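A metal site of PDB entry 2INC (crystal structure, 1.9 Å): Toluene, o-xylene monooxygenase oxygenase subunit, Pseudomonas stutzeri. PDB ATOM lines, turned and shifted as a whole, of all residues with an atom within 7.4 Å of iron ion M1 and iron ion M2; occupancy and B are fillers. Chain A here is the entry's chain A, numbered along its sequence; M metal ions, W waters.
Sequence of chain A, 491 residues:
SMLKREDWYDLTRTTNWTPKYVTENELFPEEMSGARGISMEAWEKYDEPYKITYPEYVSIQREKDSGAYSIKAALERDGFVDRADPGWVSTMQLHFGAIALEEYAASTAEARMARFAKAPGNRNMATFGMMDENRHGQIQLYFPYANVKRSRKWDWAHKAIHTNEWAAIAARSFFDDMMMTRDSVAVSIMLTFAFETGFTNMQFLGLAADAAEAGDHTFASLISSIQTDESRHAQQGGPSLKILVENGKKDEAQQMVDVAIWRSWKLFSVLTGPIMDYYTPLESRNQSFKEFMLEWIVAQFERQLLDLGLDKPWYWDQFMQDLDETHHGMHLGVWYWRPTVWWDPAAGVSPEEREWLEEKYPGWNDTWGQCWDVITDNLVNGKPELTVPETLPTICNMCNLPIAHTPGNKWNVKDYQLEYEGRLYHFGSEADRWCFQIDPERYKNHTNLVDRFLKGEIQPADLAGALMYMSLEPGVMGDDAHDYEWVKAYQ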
ATOM      1  N   ILE A  99      33.372  -3.291 -23.520  1.00  0.00           N
ATOM      2  CA  ILE A  99      32.661  -2.003 -23.426  1.00  0.00           C
ATOM      3  C   ILE A  99      31.369  -1.888 -24.228  1.00  0.00           C
ATOM      4  O   ILE A  99      30.449  -1.210 -23.783  1.00  0.00           O
ATOM      5  CB  ILE A  99      33.743  -0.893 -23.741  1.00  0.00           C
ATOM      6  CG1 ILE A  99      34.476  -0.575 -22.424  1.00  0.00           C
ATOM      7  CG2 ILE A  99      33.230   0.361 -24.424  1.00  0.00           C
ATOM      8  CD1 ILE A  99      33.643  -0.847 -21.206  1.00  0.00           C
ATOM      9  N   GLU A 102      28.187  -2.754 -22.229  1.00  0.00           N
ATOM     10  CA  GLU A 102      28.173  -1.885 -21.012  1.00  0.00           C
ATOM     11  C   GLU A 102      27.875  -0.409 -21.306  1.00  0.00           C
ATOM     12  O   GLU A 102      27.176   0.238 -20.513  1.00  0.00           O
ATOM     13  CB  GLU A 102      29.470  -2.034 -20.215  1.00  0.00           C
ATOM     14  CG  GLU A 102      29.724  -3.529 -19.696  1.00  0.00           C
ATOM     15  CD  GLU A 102      28.710  -4.017 -18.652  1.00  0.00           C
ATOM     16  OE1 GLU A 102      27.620  -3.416 -18.460  1.00  0.00           O
ATOM     17  OE2 GLU A 102      28.978  -5.023 -17.960  1.00  0.00           O
ATOM     18  N   GLU A 103      28.371   0.100 -22.433  1.00  0.00           N
ATOM     19  CA  GLU A 103      27.861   1.439 -22.972  1.00  0.00           C
ATOM     20  C   GLU A 103      26.351   1.395 -23.096  1.00  0.00           C
ATOM     21  O   GLU A 103      25.632   2.248 -22.559  1.00  0.00           O
ATOM     22  CB  GLU A 103      28.444   1.758 -24.345  1.00  0.00           C
ATOM     23  CG  GLU A 103      29.974   1.966 -24.359  1.00  0.00           C
ATOM     24  CD  GLU A 103      30.374   3.413 -24.107  1.00  0.00           C
ATOM     25  OE1 GLU A 103      29.629   4.202 -23.449  1.00  0.00           O
ATOM     26  OE2 GLU A 103      31.473   3.776 -24.565  1.00  0.00           O
ATOM     27  N   TYR A 104      25.840   0.371 -23.788  1.00  0.00           N
ATOM     28  CA  TYR A 104      24.391   0.251 -23.934  1.00  0.00           C
ATOM     29  C   TYR A 104      23.641   0.116 -22.600  1.00  0.00           C
ATOM     30  O   TYR A 104      22.572   0.759 -22.396  1.00  0.00           O
ATOM     31  CB  TYR A 104      24.032  -0.896 -24.908  1.00  0.00           C
ATOM     32  CG  TYR A 104      22.558  -0.994 -25.137  1.00  0.00           C
ATOM     33  CD1 TYR A 104      21.904  -0.102 -25.996  1.00  0.00           C
ATOM     34  CD2 TYR A 104      21.819  -2.020 -24.539  1.00  0.00           C
ATOM     35  CE1 TYR A 104      20.526  -0.210 -26.204  1.00  0.00           C
ATOM     36  CE2 TYR A 104      20.437  -2.138 -24.712  1.00  0.00           C
ATOM     37  CZ  TYR A 104      19.798  -1.240 -25.556  1.00  0.00           C
ATOM     38  OH  TYR A 104      18.434  -1.344 -25.720  1.00  0.00           O
ATOM     39  N   ALA A 106      24.620   1.402 -19.839  1.00  0.00           N
ATOM     40  CA  ALA A 106      24.674   2.758 -19.295  1.00  0.00           C
ATOM     41  C   ALA A 106      23.451   3.592 -19.734  1.00  0.00           C
ATOM     42  O   ALA A 106      23.055   4.543 -19.032  1.00  0.00           O
ATOM     43  CB  ALA A 106      25.962   3.408 -19.685  1.00  0.00           C
ATOM     44  N   GLU A 110      21.308   5.714 -17.145  1.00  0.00           N
ATOM     45  CA  GLU A 110      20.845   7.121 -17.363  1.00  0.00           C
ATOM     46  C   GLU A 110      19.306   7.178 -17.199  1.00  0.00           C
ATOM     47  O   GLU A 110      18.769   8.095 -16.560  1.00  0.00           O
ATOM     48  CB  GLU A 110      21.344   7.631 -18.724  1.00  0.00           C
ATOM     49  CG  GLU A 110      22.901   7.830 -18.782  1.00  0.00           C
ATOM     50  CD  GLU A 110      23.379   9.152 -18.107  1.00  0.00           C
ATOM     51  OE1 GLU A 110      22.500   9.989 -17.780  1.00  0.00           O
ATOM     52  OE2 GLU A 110      24.607   9.407 -17.907  1.00  0.00           O
ATOM     53  N   GLY A 129      21.753  11.951 -21.641  1.00  0.00           N
ATOM     54  CA  GLY A 129      22.713  10.844 -21.342  1.00  0.00           C
ATOM     55  C   GLY A 129      22.239   9.494 -21.855  1.00  0.00           C
ATOM     56  O   GLY A 129      23.019   8.676 -22.402  1.00  0.00           O
ATOM     57  N   ASP A 132      22.894   9.485 -25.475  1.00  0.00           N
ATOM     58  CA  ASP A 132      24.336   9.354 -25.754  1.00  0.00           C
ATOM     59  C   ASP A 132      24.870   7.916 -25.631  1.00  0.00           C
ATOM     60  O   ASP A 132      25.564   7.448 -26.511  1.00  0.00           O
ATOM     61  CB  ASP A 132      25.141  10.180 -24.738  1.00  0.00           C
ATOM     62  CG  ASP A 132      25.023  11.678 -24.963  1.00  0.00           C
ATOM     63  OD1 ASP A 132      24.612  12.088 -26.076  1.00  0.00           O
ATOM     64  OD2 ASP A 132      25.341  12.426 -23.996  1.00  0.00           O
ATOM     65  N   GLU A 133      24.509   7.232 -24.536  1.00  0.00           N
ATOM     66  CA  GLU A 133      24.943   5.836 -24.352  1.00  0.00           C
ATOM     67  C   GLU A 133      24.290   4.910 -25.356  1.00  0.00           C
ATOM     68  O   GLU A 133      24.857   3.898 -25.785  1.00  0.00           O
ATOM     69  CB  GLU A 133      24.647   5.392 -22.925  1.00  0.00           C
ATOM     70  CG  GLU A 133      25.215   6.344 -21.841  1.00  0.00           C
ATOM     71  CD  GLU A 133      26.740   6.470 -21.807  1.00  0.00           C
ATOM     72  OE1 GLU A 133      27.400   6.050 -22.747  1.00  0.00           O
ATOM     73  OE2 GLU A 133      27.308   7.020 -20.823  1.00  0.00           O
ATOM     74  N   ASN A 134      23.077   5.242 -25.764  1.00  0.00           N
ATOM     75  CA  ASN A 134      22.475   4.545 -26.913  1.00  0.00           C
ATOM     76  C   ASN A 134      23.369   4.646 -28.149  1.00  0.00           C
ATOM     77  O   ASN A 134      23.702   3.632 -28.794  1.00  0.00           O
ATOM     78  CB  ASN A 134      21.084   5.114 -27.148  1.00  0.00           C
ATOM     79  CG  ASN A 134      20.381   4.439 -28.325  1.00  0.00           C
ATOM     80  OD1 ASN A 134      20.508   4.901 -29.454  1.00  0.00           O
ATOM     81  ND2 ASN A 134      19.635   3.358 -28.059  1.00  0.00           N
ATOM     82  N   ARG A 135      23.825   5.868 -28.467  1.00  0.00           N
ATOM     83  CA  ARG A 135      24.761   6.065 -29.544  1.00  0.00           C
ATOM     84  C   ARG A 135      25.998   5.187 -29.337  1.00  0.00           C
ATOM     85  O   ARG A 135      26.447   4.472 -30.254  1.00  0.00           O
ATOM     86  CB  ARG A 135      25.231   7.498 -29.618  1.00  0.00           C
ATOM     87  CG  ARG A 135      26.309   7.733 -30.674  1.00  0.00           C
ATOM     88  CD  ARG A 135      26.752   9.156 -30.743  1.00  0.00           C
ATOM     89  NE  ARG A 135      27.583   9.355 -31.949  1.00  0.00           N
ATOM     90  CZ  ARG A 135      28.793   9.957 -31.989  1.00  0.00           C
ATOM     91  NH1 ARG A 135      29.330  10.530 -30.932  1.00  0.00           N
ATOM     92  NH2 ARG A 135      29.420  10.054 -33.144  1.00  0.00           N
ATOM     93  N   HIS A 136      26.587   5.267 -28.154  1.00  0.00           N
ATOM     94  CA  HIS A 136      27.865   4.602 -27.896  1.00  0.00           C
ATOM     95  C   HIS A 136      27.787   3.098 -28.015  1.00  0.00           C
ATOM     96  O   HIS A 136      28.716   2.487 -28.524  1.00  0.00           O
ATOM     97  CB  HIS A 136      28.459   5.040 -26.532  1.00  0.00           C
ATOM     98  CG  HIS A 136      28.687   6.534 -26.426  1.00  0.00           C
ATOM     99  ND1 HIS A 136      29.103   7.170 -25.250  1.00  0.00           N
ATOM    100  CD2 HIS A 136      28.596   7.511 -27.361  1.00  0.00           C
ATOM    101  CE1 HIS A 136      29.186   8.464 -25.473  1.00  0.00           C
ATOM    102  NE2 HIS A 136      28.927   8.699 -26.752  1.00  0.00           N
ATOM    103  N   GLY A 137      26.706   2.519 -27.551  1.00  0.00           N
ATOM    104  CA  GLY A 137      26.548   1.096 -27.606  1.00  0.00           C
ATOM    105  C   GLY A 137      26.379   0.758 -29.067  1.00  0.00           C
ATOM    106  O   GLY A 137      26.978  -0.207 -29.554  1.00  0.00           O
ATOM    107  N   GLN A 140      29.685   1.331 -31.330  1.00  0.00           N
ATOM    108  CA  GLN A 140      30.726   0.400 -30.918  1.00  0.00           C
ATOM    109  C   GLN A 140      30.326  -1.044 -31.199  1.00  0.00           C
ATOM    110  O   GLN A 140      31.079  -1.986 -30.885  1.00  0.00           O
ATOM    111  CB  GLN A 140      31.128   0.599 -29.462  1.00  0.00           C
ATOM    112  CG  GLN A 140      31.933   1.938 -29.472  1.00  0.00           C
ATOM    113  CD  GLN A 140      32.484   2.359 -28.118  1.00  0.00           C
ATOM    114  OE1 GLN A 140      33.684   2.309 -27.908  1.00  0.00           O
ATOM    115  NE2 GLN A 140      31.611   2.755 -27.219  1.00  0.00           N
ATOM    116  N   LEU A 191      28.640   6.569 -11.174  1.00  0.00           N
ATOM    117  CA  LEU A 191      28.872   6.524 -12.627  1.00  0.00           C
ATOM    118  C   LEU A 191      29.424   7.869 -13.187  1.00  0.00           C
ATOM    119  O   LEU A 191      30.550   7.933 -13.727  1.00  0.00           O
ATOM    120  CB  LEU A 191      27.575   6.125 -13.355  1.00  0.00           C
ATOM    121  CG  LEU A 191      27.577   6.115 -14.885  1.00  0.00           C
ATOM    122  CD1 LEU A 191      28.673   5.167 -15.399  1.00  0.00           C
ATOM    123  CD2 LEU A 191      26.188   5.839 -15.524  1.00  0.00           C
ATOM    124  N   THR A 192      28.643   8.945 -13.082  1.00  0.00           N
ATOM    125  CA  THR A 192      28.985  10.089 -13.893  1.00  0.00           C
ATOM    126  C   THR A 192      30.159  10.885 -13.323  1.00  0.00           C
ATOM    127  O   THR A 192      30.991  11.344 -14.095  1.00  0.00           O
ATOM    128  CB  THR A 192      27.771  11.004 -14.252  1.00  0.00           C
ATOM    129  OG1 THR A 192      27.345  11.721 -13.100  1.00  0.00           O
ATOM    130  CG2 THR A 192      26.573  10.221 -14.757  1.00  0.00           C
ATOM    131  N   PHE A 195      33.401   7.600 -12.245  1.00  0.00           N
ATOM    132  CA  PHE A 195      33.911   6.847 -13.379  1.00  0.00           C
ATOM    133  C   PHE A 195      34.045   7.672 -14.654  1.00  0.00           C
ATOM    134  O   PHE A 195      35.049   7.572 -15.377  1.00  0.00           O
ATOM    135  CB  PHE A 195      32.991   5.639 -13.663  1.00  0.00           C
ATOM    136  CG  PHE A 195      33.494   4.711 -14.759  1.00  0.00           C
ATOM    137  CD1 PHE A 195      34.688   3.997 -14.613  1.00  0.00           C
ATOM    138  CD2 PHE A 195      32.749   4.513 -15.899  1.00  0.00           C
ATOM    139  CE1 PHE A 195      35.139   3.115 -15.605  1.00  0.00           C
ATOM    140  CE2 PHE A 195      33.198   3.648 -16.889  1.00  0.00           C
ATOM    141  CZ  PHE A 195      34.370   2.936 -16.737  1.00  0.00           C
ATOM    142  N   GLU A 196      33.021   8.431 -15.028  1.00  0.00           N
ATOM    143  CA  GLU A 196      33.066   9.060 -16.361  1.00  0.00           C
ATOM    144  C   GLU A 196      33.903  10.346 -16.318  1.00  0.00           C
ATOM    145  O   GLU A 196      34.863  10.546 -17.109  1.00  0.00           O
ATOM    146  CB  GLU A 196      31.642   9.339 -16.904  1.00  0.00           C
ATOM    147  CG  GLU A 196      30.806   8.078 -17.235  1.00  0.00           C
ATOM    148  CD  GLU A 196      29.420   8.412 -17.808  1.00  0.00           C
ATOM    149  OE1 GLU A 196      28.710   9.183 -17.152  1.00  0.00           O
ATOM    150  OE2 GLU A 196      29.017   7.910 -18.891  1.00  0.00           O
ATOM    151  N   THR A 200      37.072   7.985 -17.604  1.00  0.00           N
ATOM    152  CA  THR A 200      36.943   7.681 -19.039  1.00  0.00           C
ATOM    153  C   THR A 200      37.069   8.912 -19.944  1.00  0.00           C
ATOM    154  O   THR A 200      37.405   8.784 -21.120  1.00  0.00           O
ATOM    155  CB  THR A 200      35.638   6.940 -19.377  1.00  0.00           C
ATOM    156  OG1 THR A 200      34.542   7.769 -19.075  1.00  0.00           O
ATOM    157  CG2 THR A 200      35.496   5.725 -18.542  1.00  0.00           C
ATOM    158  N   PHE A 204      39.691   8.311 -22.854  1.00  0.00           N
ATOM    159  CA  PHE A 204      39.323   8.266 -24.265  1.00  0.00           C
ATOM    160  C   PHE A 204      40.142   9.227 -25.132  1.00  0.00           C
ATOM    161  O   PHE A 204      40.402   8.942 -26.283  1.00  0.00           O
ATOM    162  CB  PHE A 204      37.809   8.491 -24.438  1.00  0.00           C
ATOM    163  CG  PHE A 204      36.996   7.223 -24.386  1.00  0.00           C
ATOM    164  CD1 PHE A 204      37.306   6.195 -23.475  1.00  0.00           C
ATOM    165  CD2 PHE A 204      35.886   7.054 -25.237  1.00  0.00           C
ATOM    166  CE1 PHE A 204      36.542   4.983 -23.444  1.00  0.00           C
ATOM    167  CE2 PHE A 204      35.120   5.859 -25.190  1.00  0.00           C
ATOM    168  CZ  PHE A 204      35.447   4.822 -24.280  1.00  0.00           C
ATOM    169  N   ILE A 226      33.124   9.881 -29.621  1.00  0.00           N
ATOM    170  CA  ILE A 226      32.402   9.410 -28.458  1.00  0.00           C
ATOM    171  C   ILE A 226      32.819  10.257 -27.331  1.00  0.00           C
ATOM    172  O   ILE A 226      32.021  10.608 -26.507  1.00  0.00           O
ATOM    173  CB  ILE A 226      32.895   7.957 -28.038  1.00  0.00           C
ATOM    174  CG1 ILE A 226      32.374   6.885 -28.964  1.00  0.00           C
ATOM    175  CG2 ILE A 226      32.556   7.650 -26.575  1.00  0.00           C
ATOM    176  CD1 ILE A 226      31.382   7.394 -29.932  1.00  0.00           C
ATOM    177  N   ASP A 229      31.047  13.489 -26.417  1.00  0.00           N
ATOM    178  CA  ASP A 229      29.699  13.377 -25.821  1.00  0.00           C
ATOM    179  C   ASP A 229      29.753  13.298 -24.314  1.00  0.00           C
ATOM    180  O   ASP A 229      28.746  13.513 -23.686  1.00  0.00           O
ATOM    181  CB  ASP A 229      28.985  12.102 -26.280  1.00  0.00           C
ATOM    182  CG  ASP A 229      28.663  12.087 -27.744  1.00  0.00           C
ATOM    183  OD1 ASP A 229      28.453  13.137 -28.374  1.00  0.00           O
ATOM    184  OD2 ASP A 229      28.592  10.971 -28.299  1.00  0.00           O
ATOM    185  N   GLU A 230      30.897  12.879 -23.754  1.00  0.00           N
ATOM    186  CA  GLU A 230      31.015  12.488 -22.371  1.00  0.00           C
ATOM    187  C   GLU A 230      30.634  13.559 -21.387  1.00  0.00           C
ATOM    188  O   GLU A 230      29.790  13.316 -20.521  1.00  0.00           O
ATOM    189  CB  GLU A 230      32.424  11.924 -22.043  1.00  0.00           C
ATOM    190  CG  GLU A 230      32.419  11.044 -20.779  1.00  0.00           C
ATOM    191  CD  GLU A 230      31.735   9.702 -21.060  1.00  0.00           C
ATOM    192  OE1 GLU A 230      32.000   9.106 -22.145  1.00  0.00           O
ATOM    193  OE2 GLU A 230      30.920   9.250 -20.223  1.00  0.00           O
ATOM    194  N   SER A 231      31.209  14.756 -21.514  1.00  0.00           N
ATOM    195  CA  SER A 231      30.961  15.754 -20.479  1.00  0.00           C
ATOM    196  C   SER A 231      29.466  16.177 -20.375  1.00  0.00           C
ATOM    197  O   SER A 231      28.979  16.504 -19.308  1.00  0.00           O
ATOM    198  CB  SER A 231      31.859  16.956 -20.672  1.00  0.00           C
ATOM    199  OG  SER A 231      31.391  17.660 -21.805  1.00  0.00           O
ATOM    200  N   HIS A 233      26.980  14.464 -20.122  1.00  0.00           N
ATOM    201  CA  HIS A 233      26.262  13.652 -19.130  1.00  0.00           C
ATOM    202  C   HIS A 233      27.105  13.341 -17.922  1.00  0.00           C
ATOM    203  O   HIS A 233      26.573  13.085 -16.897  1.00  0.00           O
ATOM    204  CB  HIS A 233      25.610  12.402 -19.735  1.00  0.00           C
ATOM    205  CG  HIS A 233      26.577  11.425 -20.332  1.00  0.00           C
ATOM    206  ND1 HIS A 233      26.832  11.348 -21.681  1.00  0.00           N
ATOM    207  CD2 HIS A 233      27.372  10.478 -19.747  1.00  0.00           C
ATOM    208  CE1 HIS A 233      27.726  10.397 -21.906  1.00  0.00           C
ATOM    209  NE2 HIS A 233      28.061   9.852 -20.744  1.00  0.00           N
ATOM    210  N   ALA A 234      28.435  13.400 -18.048  1.00  0.00           N
ATOM    211  CA  ALA A 234      29.333  13.097 -16.944  1.00  0.00           C
ATOM    212  C   ALA A 234      29.226  14.176 -15.906  1.00  0.00           C
ATOM    213  O   ALA A 234      29.489  13.936 -14.740  1.00  0.00           O
ATOM    214  CB  ALA A 234      30.733  13.015 -17.461  1.00  0.00           C
HETATM  215 FE    FE M   1      29.160   8.003 -20.679  1.00  0.00          FE
HETATM  216 FE    FE M   2      29.500   6.274 -23.228  1.00  0.00          FE
HETATM  217  O   HOH W   1      31.723   6.266 -23.605  1.00  0.00           O
HETATM  218  O   HOH W   2      29.803   8.179 -22.387  1.00  0.00           O
HETATM  219  O   HOH W   3      29.951   5.849 -20.907  1.00  0.00           O
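Water W1 lies within hydrogen-bond range of OE2 of Glu 103 (2.7 Å) and OE1 of Glu 230 (3.2 Å).
O of Glu 196 sits close to OG1 of Thr 200, 3.4 Å away. The backbone NH (N) of Glu 196 lies within hydrogen-bond range of the backbone carbonyl oxygen (O) of Leu 191 (2.8 Å). OE2 of Glu 103 sits at hydrogen-bond distance from NE2 of Gln 140, 2.8 Å away. OD2 of Asp 132 is in hydrogen-bond range of ND1 of His 233, 3.0 Å away. The backbone carbonyl oxygen (O) of His 136 sits at hydrogen-bond distance from the side-chain amide nitrogen (NE2) of Gln 140 (3.2 Å). The side-chain carboxylate (OD2) of Asp 229 is in hydrogen-bond range of a ring nitrogen (NE2) of His 136, 2.8 Å away.
Of the 26 residues printed, 4 come within 4 Å of iron ion M1. The nearest printed residue that does not touch iron ion M1 is His 136 (4.6 Å).
Iron ion M2 is bound by the side-chain carboxylate (OE1) of Glu 103 (2.1 Å), water W2 (2.1 Å), the side-chain carboxylate (OE1) of Glu 133 (2.2 Å), a ring nitrogen (ND1) of His 136 (2.2 Å), water W1 (2.3 Å) and water W3 (2.4 Å). Iron ion M2 has six donor atoms within binding distance.
Iron ion M1 is bound by the side-chain carboxylate (OE2) of Glu 196 (1.8 Å), water W2 (1.8 Å), the side-chain carboxylate (OE2) of Glu 133 (2.1 Å), a ring nitrogen (NE2) of His 233 (2.2 Å), the side-chain carboxylate (OE2) of Glu 230 (2.2 Å) and water W3 (2.3 Å). Iron ion M1 has six donor atoms within binding distance.
Four residues have an atom within 4 Å of iron ion M2: Glu 103, Glu 133, His 136 and Glu 230. The nearest printed residue that does not touch iron ion M2 is His 233 (4.6 Å).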
